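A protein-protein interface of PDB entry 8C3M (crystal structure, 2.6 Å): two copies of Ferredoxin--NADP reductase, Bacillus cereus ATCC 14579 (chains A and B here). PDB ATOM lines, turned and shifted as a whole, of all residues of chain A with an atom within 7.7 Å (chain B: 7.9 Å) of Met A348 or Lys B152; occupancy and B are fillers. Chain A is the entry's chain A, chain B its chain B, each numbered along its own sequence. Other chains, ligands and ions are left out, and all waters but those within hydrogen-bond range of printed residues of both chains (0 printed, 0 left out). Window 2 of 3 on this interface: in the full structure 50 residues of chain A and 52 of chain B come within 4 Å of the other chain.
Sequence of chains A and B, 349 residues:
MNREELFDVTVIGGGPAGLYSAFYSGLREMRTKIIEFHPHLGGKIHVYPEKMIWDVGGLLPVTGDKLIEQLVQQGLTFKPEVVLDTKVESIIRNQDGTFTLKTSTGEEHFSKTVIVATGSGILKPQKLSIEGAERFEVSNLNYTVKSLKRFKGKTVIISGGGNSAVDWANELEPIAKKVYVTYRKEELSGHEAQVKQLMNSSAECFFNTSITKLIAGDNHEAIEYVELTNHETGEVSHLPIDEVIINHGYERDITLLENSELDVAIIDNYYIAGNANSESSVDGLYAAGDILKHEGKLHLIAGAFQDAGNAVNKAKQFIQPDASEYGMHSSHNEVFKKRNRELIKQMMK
The backbone carbonyl oxygen (O) of Met A347 sits at hydrogen-bond distance from the side-chain amino group (NZ) of Lys B149, 3.2 Å away. The backbone carbonyl oxygen (O) of Met A348 sits close to the side-chain amino group (NZ) of Lys B152, at 2.4 Å.
The backbone NH (N) of Lys B149 lies close to the side-chain hydroxyl (OG) of Ser B147.
Among the printed residues, merely in contact across the chains: Met A348 with Lys B149, Lys A349 with Lys B149 and Ile A344 with Leu B148.
Met A348 touches two residues of chain B. Lys B152 touches just one residue of chain A: Met A348. Of the printed residues of chain A, Lys B149 touches Met A347, Met A348 and Lys A349. Printed residues of chain B within 4 Å of Lys A349: Lys B149 (3.7 Å). Of the printed residues of chain B, Ile A344 touches Leu B148 (3.8 Å). Printed residues of chain A within 4 Å of Leu B148: Ile A344 (3.8 Å). Printed residues of chain B within 4 Å of Met A347: Lys B149. Val B156 touches none of the printed residues of chain A. Asp B242 touches none of the printed residues of chain A. The nearest residue of chain B that does not touch Met A348 is Leu B148 (4.1 Å).
Hydrophobic or aromatic side chains of chain A that line the printed part of chain B: Ile A344 and Met A348. Along chain A the printed residues that touch a printed residue of chain B span positions 344 to 349. Among the printed residues, 5 pairs touch across the chains. Among the printed residues, no Asp or Glu carboxylate lies within 4 Å of a Lys or Arg side-chain nitrogen of the other chain.
No position is printed for both chains. Of the 5 pairs that touch across the chains among the printed residues, none has its exchanged pair printed and touching as well.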
ATOM      1  N   GLU A 342       5.176   0.850   0.127  1.00  0.00           N
ATOM      2  CA  GLU A 342       6.305  -0.003   0.458  1.00  0.00           C
ATOM      3  C   GLU A 342       7.562   0.835   0.695  1.00  0.00           C
ATOM      4  O   GLU A 342       8.297   0.589   1.657  1.00  0.00           O
ATOM      5  CB  GLU A 342       6.492  -1.040  -0.663  1.00  0.00           C
ATOM      6  CG  GLU A 342       7.639  -2.034  -0.476  1.00  0.00           C
ATOM      7  CD  GLU A 342       7.339  -3.141   0.532  1.00  0.00           C
ATOM      8  OE1 GLU A 342       6.166  -3.270   0.975  1.00  0.00           O
ATOM      9  OE2 GLU A 342       8.289  -3.881   0.891  1.00  0.00           O
ATOM     10  N   LEU A 343       7.787   1.865  -0.144  1.00  0.00           N
ATOM     11  CA  LEU A 343       8.957   2.739  -0.015  1.00  0.00           C
ATOM     12  C   LEU A 343       8.967   3.511   1.302  1.00  0.00           C
ATOM     13  O   LEU A 343      10.020   3.671   1.931  1.00  0.00           O
ATOM     14  CB  LEU A 343       8.993   3.722  -1.171  1.00  0.00           C
ATOM     15  CG  LEU A 343       9.349   3.228  -2.571  1.00  0.00           C
ATOM     16  CD1 LEU A 343       9.289   4.399  -3.567  1.00  0.00           C
ATOM     17  CD2 LEU A 343      10.690   2.549  -2.645  1.00  0.00           C
ATOM     18  N   ILE A 344       7.812   4.034   1.714  1.00  0.00           N
ATOM     19  CA  ILE A 344       7.728   4.778   2.968  1.00  0.00           C
ATOM     20  C   ILE A 344       7.969   3.846   4.149  1.00  0.00           C
ATOM     21  O   ILE A 344       8.558   4.241   5.164  1.00  0.00           O
ATOM     22  CB  ILE A 344       6.365   5.493   3.092  1.00  0.00           C
ATOM     23  CG1 ILE A 344       6.130   6.474   1.941  1.00  0.00           C
ATOM     24  CG2 ILE A 344       6.235   6.194   4.449  1.00  0.00           C
ATOM     25  CD1 ILE A 344       7.330   7.333   1.589  1.00  0.00           C
ATOM     26  N   LYS A 345       7.481   2.608   4.060  1.00  0.00           N
ATOM     27  CA  LYS A 345       7.729   1.666   5.140  1.00  0.00           C
ATOM     28  C   LYS A 345       9.219   1.372   5.292  1.00  0.00           C
ATOM     29  O   LYS A 345       9.692   1.120   6.404  1.00  0.00           O
ATOM     30  CB  LYS A 345       6.937   0.382   4.914  1.00  0.00           C
ATOM     31  CG  LYS A 345       7.012  -0.573   6.064  1.00  0.00           C
ATOM     32  CD  LYS A 345       6.354  -0.052   7.346  1.00  0.00           C
ATOM     33  CE  LYS A 345       4.816  -0.068   7.307  1.00  0.00           C
ATOM     34  NZ  LYS A 345       4.219  -0.330   8.696  1.00  0.00           N
ATOM     35  N   GLN A 346       9.981   1.410   4.193  1.00  0.00           N
ATOM     36  CA  GLN A 346      11.426   1.241   4.315  1.00  0.00           C
ATOM     37  C   GLN A 346      12.115   2.521   4.791  1.00  0.00           C
ATOM     38  O   GLN A 346      13.124   2.442   5.501  1.00  0.00           O
ATOM     39  CB  GLN A 346      12.011   0.787   2.972  1.00  0.00           C
ATOM     40  CG  GLN A 346      13.095  -0.271   3.108  1.00  0.00           C
ATOM     41  CD  GLN A 346      12.573  -1.507   3.820  1.00  0.00           C
ATOM     42  OE1 GLN A 346      11.468  -1.978   3.531  1.00  0.00           O
ATOM     43  NE2 GLN A 346      13.348  -2.023   4.774  1.00  0.00           N
ATOM     44  N   MET A 347      11.553   3.698   4.468  1.00  0.00           N
ATOM     45  CA  MET A 347      12.136   4.979   4.879  1.00  0.00           C
ATOM     46  C   MET A 347      12.037   5.211   6.387  1.00  0.00           C
ATOM     47  O   MET A 347      12.840   5.966   6.946  1.00  0.00           O
ATOM     48  CB  MET A 347      11.451   6.135   4.140  1.00  0.00           C
ATOM     49  CG  MET A 347      12.076   6.496   2.806  1.00  0.00           C
ATOM     50  SD  MET A 347      11.407   8.009   2.058  1.00  0.00           S
ATOM     51  CE  MET A 347      11.647   9.151   3.434  1.00  0.00           C
ATOM     52  N   MET A 348      11.053   4.614   7.057  1.00  0.00           N
ATOM     53  CA  MET A 348      10.925   4.790   8.500  1.00  0.00           C
ATOM     54  C   MET A 348      11.816   3.831   9.271  1.00  0.00           C
ATOM     55  O   MET A 348      11.515   3.527  10.429  1.00  0.00           O
ATOM     56  CB  MET A 348       9.475   4.591   8.953  1.00  0.00           C
ATOM     57  CG  MET A 348       8.447   5.382   8.171  1.00  0.00           C
ATOM     58  SD  MET A 348       8.542   7.171   8.416  1.00  0.00           S
ATOM     59  CE  MET A 348       9.393   7.690   6.933  1.00  0.00           C
ATOM     60  N   LYS A 349      12.919   3.388   8.659  1.00  0.00           N
ATOM     61  CA  LYS A 349      13.709   2.240   9.126  1.00  0.00           C
ATOM     62  C   LYS A 349      12.877   0.965   8.885  1.00  0.00           C
ATOM     63  O   LYS A 349      11.673   0.897   9.142  1.00  0.00           O
ATOM     64  CB  LYS A 349      14.122   2.418  10.608  1.00  0.00           C
ATOM     65  CG  LYS A 349      14.464   1.154  11.419  1.00  0.00           C
ATOM     66  CD  LYS A 349      15.776   0.476  11.041  1.00  0.00           C
ATOM     67  CE  LYS A 349      16.004  -0.742  11.929  1.00  0.00           C
ATOM     68  NZ  LYS A 349      17.192  -1.540  11.525  1.00  0.00           N
ATOM     69  OXT LYS A 349      13.378  -0.049   8.395  1.00  0.00           O
ATOM     70  N   SER B 147       9.444  16.335   5.735  1.00  0.00           N
ATOM     71  CA  SER B 147       9.697  14.926   5.469  1.00  0.00           C
ATOM     72  C   SER B 147       8.763  14.110   6.347  1.00  0.00           C
ATOM     73  O   SER B 147       8.406  14.536   7.450  1.00  0.00           O
ATOM     74  CB  SER B 147      11.142  14.533   5.759  1.00  0.00           C
ATOM     75  OG  SER B 147      11.266  14.197   7.116  1.00  0.00           O
ATOM     76  N   LEU B 148       8.374  12.933   5.846  1.00  0.00           N
ATOM     77  CA  LEU B 148       7.517  12.059   6.637  1.00  0.00           C
ATOM     78  C   LEU B 148       8.237  11.577   7.892  1.00  0.00           C
ATOM     79  O   LEU B 148       7.627  11.456   8.958  1.00  0.00           O
ATOM     80  CB  LEU B 148       7.069  10.877   5.784  1.00  0.00           C
ATOM     81  CG  LEU B 148       6.118  11.172   4.622  1.00  0.00           C
ATOM     82  CD1 LEU B 148       5.738   9.902   3.924  1.00  0.00           C
ATOM     83  CD2 LEU B 148       4.874  11.891   5.102  1.00  0.00           C
ATOM     84  N   LYS B 149       9.549  11.321   7.795  1.00  0.00           N
ATOM     85  CA  LYS B 149      10.273  10.795   8.948  1.00  0.00           C
ATOM     86  C   LYS B 149      10.340  11.801  10.076  1.00  0.00           C
ATOM     87  O   LYS B 149      10.261  11.416  11.245  1.00  0.00           O
ATOM     88  CB  LYS B 149      11.690  10.364   8.571  1.00  0.00           C
ATOM     89  CG  LYS B 149      12.236   9.336   9.543  1.00  0.00           C
ATOM     90  CD  LYS B 149      13.360   8.518   8.948  1.00  0.00           C
ATOM     91  CE  LYS B 149      13.722   7.349   9.874  1.00  0.00           C
ATOM     92  NZ  LYS B 149      14.851   6.514   9.351  1.00  0.00           N
ATOM     93  N   ARG B 150      10.413  13.090   9.747  1.00  0.00           N
ATOM     94  CA  ARG B 150      10.456  14.123  10.772  1.00  0.00           C
ATOM     95  C   ARG B 150       9.344  13.932  11.807  1.00  0.00           C
ATOM     96  O   ARG B 150       9.520  14.279  12.983  1.00  0.00           O
ATOM     97  CB  ARG B 150      10.336  15.495  10.091  1.00  0.00           C
ATOM     98  CG  ARG B 150      10.855  16.664  10.883  1.00  0.00           C
ATOM     99  CD  ARG B 150       9.759  17.615  11.329  1.00  0.00           C
ATOM    100  NE  ARG B 150      10.288  18.927  11.712  1.00  0.00           N
ATOM    101  CZ  ARG B 150      10.821  19.219  12.896  1.00  0.00           C
ATOM    102  NH1 ARG B 150      10.948  18.303  13.842  1.00  0.00           N
ATOM    103  NH2 ARG B 150      11.216  20.467  13.142  1.00  0.00           N
ATOM    104  N   PHE B 151       8.223  13.331  11.403  1.00  0.00           N
ATOM    105  CA  PHE B 151       7.041  13.236  12.247  1.00  0.00           C
ATOM    106  C   PHE B 151       6.789  11.829  12.752  1.00  0.00           C
ATOM    107  O   PHE B 151       5.784  11.600  13.436  1.00  0.00           O
ATOM    108  CB  PHE B 151       5.800  13.747  11.493  1.00  0.00           C
ATOM    109  CG  PHE B 151       5.915  15.176  11.064  1.00  0.00           C
ATOM    110  CD1 PHE B 151       5.516  16.197  11.910  1.00  0.00           C
ATOM    111  CD2 PHE B 151       6.456  15.497   9.827  1.00  0.00           C
ATOM    112  CE1 PHE B 151       5.643  17.511  11.527  1.00  0.00           C
ATOM    113  CE2 PHE B 151       6.582  16.802   9.440  1.00  0.00           C
ATOM    114  CZ  PHE B 151       6.177  17.816  10.286  1.00  0.00           C
ATOM    115  N   LYS B 152       7.679  10.891  12.449  1.00  0.00           N
ATOM    116  CA  LYS B 152       7.495   9.520  12.890  1.00  0.00           C
ATOM    117  C   LYS B 152       7.366   9.479  14.403  1.00  0.00           C
ATOM    118  O   LYS B 152       8.207  10.021  15.129  1.00  0.00           O
ATOM    119  CB  LYS B 152       8.671   8.665  12.432  1.00  0.00           C
ATOM    120  CG  LYS B 152       8.608   7.222  12.877  1.00  0.00           C
ATOM    121  CD  LYS B 152       9.891   6.492  12.513  1.00  0.00           C
ATOM    122  CE  LYS B 152       9.940   5.098  13.107  1.00  0.00           C
ATOM    123  NZ  LYS B 152      11.123   4.342  12.619  1.00  0.00           N
ATOM    124  N   GLY B 153       6.279   8.869  14.871  1.00  0.00           N
ATOM    125  CA  GLY B 153       6.023   8.699  16.286  1.00  0.00           C
ATOM    126  C   GLY B 153       5.810   9.971  17.067  1.00  0.00           C
ATOM    127  O   GLY B 153       5.906   9.945  18.295  1.00  0.00           O
ATOM    128  N   LYS B 154       5.486  11.078  16.404  1.00  0.00           N
ATOM    129  CA  LYS B 154       5.300  12.360  17.065  1.00  0.00           C
ATOM    130  C   LYS B 154       3.828  12.751  17.073  1.00  0.00           C
ATOM    131  O   LYS B 154       3.018  12.224  16.307  1.00  0.00           O
ATOM    132  CB  LYS B 154       6.126  13.458  16.384  1.00  0.00           C
ATOM    133  CG  LYS B 154       7.638  13.292  16.537  1.00  0.00           C
ATOM    134  CD  LYS B 154       8.294  14.641  16.845  1.00  0.00           C
ATOM    135  CE  LYS B 154       9.820  14.568  16.816  1.00  0.00           C
ATOM    136  NZ  LYS B 154      10.425  15.349  15.687  1.00  0.00           N
ATOM    137  N   THR B 155       3.498  13.713  17.933  1.00  0.00           N
ATOM    138  CA  THR B 155       2.138  14.223  18.079  1.00  0.00           C
ATOM    139  C   THR B 155       2.051  15.578  17.395  1.00  0.00           C
ATOM    140  O   THR B 155       2.691  16.539  17.838  1.00  0.00           O
ATOM    141  CB  THR B 155       1.751  14.373  19.550  1.00  0.00           C
ATOM    142  OG1 THR B 155       1.600  13.081  20.139  1.00  0.00           O
ATOM    143  CG2 THR B 155       0.448  15.154  19.693  1.00  0.00           C
ATOM    144  N   VAL B 156       1.219  15.661  16.358  1.00  0.00           N
ATOM    145  CA  VAL B 156       1.184  16.801  15.453  1.00  0.00           C
ATOM    146  C   VAL B 156      -0.200  17.416  15.492  1.00  0.00           C
ATOM    147  O   VAL B 156      -1.204  16.701  15.433  1.00  0.00           O
ATOM    148  CB  VAL B 156       1.501  16.369  14.008  1.00  0.00           C
ATOM    149  CG1 VAL B 156       1.669  17.590  13.104  1.00  0.00           C
ATOM    150  CG2 VAL B 156       2.703  15.459  13.968  1.00  0.00           C
ATOM    151  N   GLU B 171      -1.454  11.548   5.086  1.00  0.00           N
ATOM    152  CA  GLU B 171      -0.162  10.894   4.952  1.00  0.00           C
ATOM    153  C   GLU B 171       0.625  10.860   6.256  1.00  0.00           C
ATOM    154  O   GLU B 171       1.609  10.121   6.347  1.00  0.00           O
ATOM    155  CB  GLU B 171       0.661  11.594   3.875  1.00  0.00           C
ATOM    156  CG  GLU B 171       0.986  13.027   4.210  1.00  0.00           C
ATOM    157  CD  GLU B 171       1.859  13.694   3.166  1.00  0.00           C
ATOM    158  OE1 GLU B 171       2.235  13.023   2.170  1.00  0.00           O
ATOM    159  OE2 GLU B 171       2.171  14.890   3.351  1.00  0.00           O
ATOM    160  N   LEU B 172       0.218  11.637   7.260  1.00  0.00           N
ATOM    161  CA  LEU B 172       0.815  11.557   8.580  1.00  0.00           C
ATOM    162  C   LEU B 172       0.049  10.649   9.528  1.00  0.00           C
ATOM    163  O   LEU B 172       0.618  10.219  10.537  1.00  0.00           O
ATOM    164  CB  LEU B 172       0.918  12.949   9.198  1.00  0.00           C
ATOM    165  CG  LEU B 172       1.856  13.922   8.487  1.00  0.00           C
ATOM    166  CD1 LEU B 172       1.981  15.206   9.273  1.00  0.00           C
ATOM    167  CD2 LEU B 172       3.206  13.279   8.269  1.00  0.00           C
ATOM    168  N   PRO B 174      -0.694   7.414   9.273  1.00  0.00           N
ATOM    169  CA  PRO B 174       0.010   6.151   9.528  1.00  0.00           C
ATOM    170  C   PRO B 174       1.447   6.319  10.006  1.00  0.00           C
ATOM    171  O   PRO B 174       2.136   5.311  10.199  1.00  0.00           O
ATOM    172  CB  PRO B 174      -0.026   5.455   8.162  1.00  0.00           C
ATOM    173  CG  PRO B 174      -0.224   6.539   7.158  1.00  0.00           C
ATOM    174  CD  PRO B 174      -0.566   7.813   7.860  1.00  0.00           C
ATOM    175  N   ILE B 175       1.906   7.550  10.227  1.00  0.00           N
ATOM    176  CA  ILE B 175       3.280   7.827  10.610  1.00  0.00           C
ATOM    177  C   ILE B 175       3.368   8.445  11.999  1.00  0.00           C
ATOM    178  O   ILE B 175       4.227   8.066  12.802  1.00  0.00           O
ATOM    179  CB  ILE B 175       3.948   8.745   9.560  1.00  0.00           C
ATOM    180  CG1 ILE B 175       4.283   7.934   8.321  1.00  0.00           C
ATOM    181  CG2 ILE B 175       5.177   9.476  10.107  1.00  0.00           C
ATOM    182  CD1 ILE B 175       4.608   8.778   7.173  1.00  0.00           C
ATOM    183  N   ALA B 176       2.494   9.397  12.301  1.00  0.00           N
ATOM    184  CA  ALA B 176       2.574  10.117  13.556  1.00  0.00           C
ATOM    185  C   ALA B 176       2.024   9.266  14.691  1.00  0.00           C
ATOM    186  O   ALA B 176       1.349   8.255  14.479  1.00  0.00           O
ATOM    187  CB  ALA B 176       1.802  11.429  13.463  1.00  0.00           C
ATOM    188  N   LYS B 177       2.340   9.671  15.916  1.00  0.00           N
ATOM    189  CA  LYS B 177       1.683   9.028  17.041  1.00  0.00           C
ATOM    190  C   LYS B 177       0.207   9.407  17.080  1.00  0.00           C
ATOM    191  O   LYS B 177      -0.659   8.558  17.324  1.00  0.00           O
ATOM    192  CB  LYS B 177       2.363   9.410  18.359  1.00  0.00           C
ATOM    193  CG  LYS B 177       2.030   8.443  19.493  1.00  0.00           C
ATOM    194  CD  LYS B 177       2.700   8.848  20.804  1.00  0.00           C
ATOM    195  CE  LYS B 177       4.209   8.635  20.790  1.00  0.00           C
ATOM    196  NZ  LYS B 177       4.751   8.816  22.191  1.00  0.00           N
ATOM    197  N   ASP B 242       4.218  17.538  19.850  1.00  0.00           N
ATOM    198  CA  ASP B 242       5.619  17.528  19.462  1.00  0.00           C
ATOM    199  C   ASP B 242       5.887  18.430  18.259  1.00  0.00           C
ATOM    200  O   ASP B 242       6.996  18.959  18.116  1.00  0.00           O
ATOM    201  CB  ASP B 242       6.050  16.104  19.116  1.00  0.00           C
ATOM    202  CG  ASP B 242       5.713  15.098  20.204  1.00  0.00           C
ATOM    203  OD1 ASP B 242       5.989  15.331  21.414  1.00  0.00           O
ATOM    204  OD2 ASP B 242       5.122  14.050  19.845  1.00  0.00           O
ATOM    205  N   GLU B 243       4.920  18.574  17.361  1.00  0.00           N
ATOM    206  CA  GLU B 243       5.101  19.347  16.138  1.00  0.00           C
ATOM    207  C   GLU B 243       3.833  20.129  15.855  1.00  0.00           C
ATOM    208  O   GLU B 243       2.730  19.656  16.142  1.00  0.00           O
ATOM    209  CB  GLU B 243       5.421  18.450  14.931  1.00  0.00           C
ATOM    210  CG  GLU B 243       6.621  17.535  15.142  1.00  0.00           C
ATOM    211  CD  GLU B 243       7.951  18.195  14.800  1.00  0.00           C
ATOM    212  OE1 GLU B 243       7.945  19.364  14.339  1.00  0.00           O
ATOM    213  OE2 GLU B 243       9.006  17.545  15.012  1.00  0.00           O
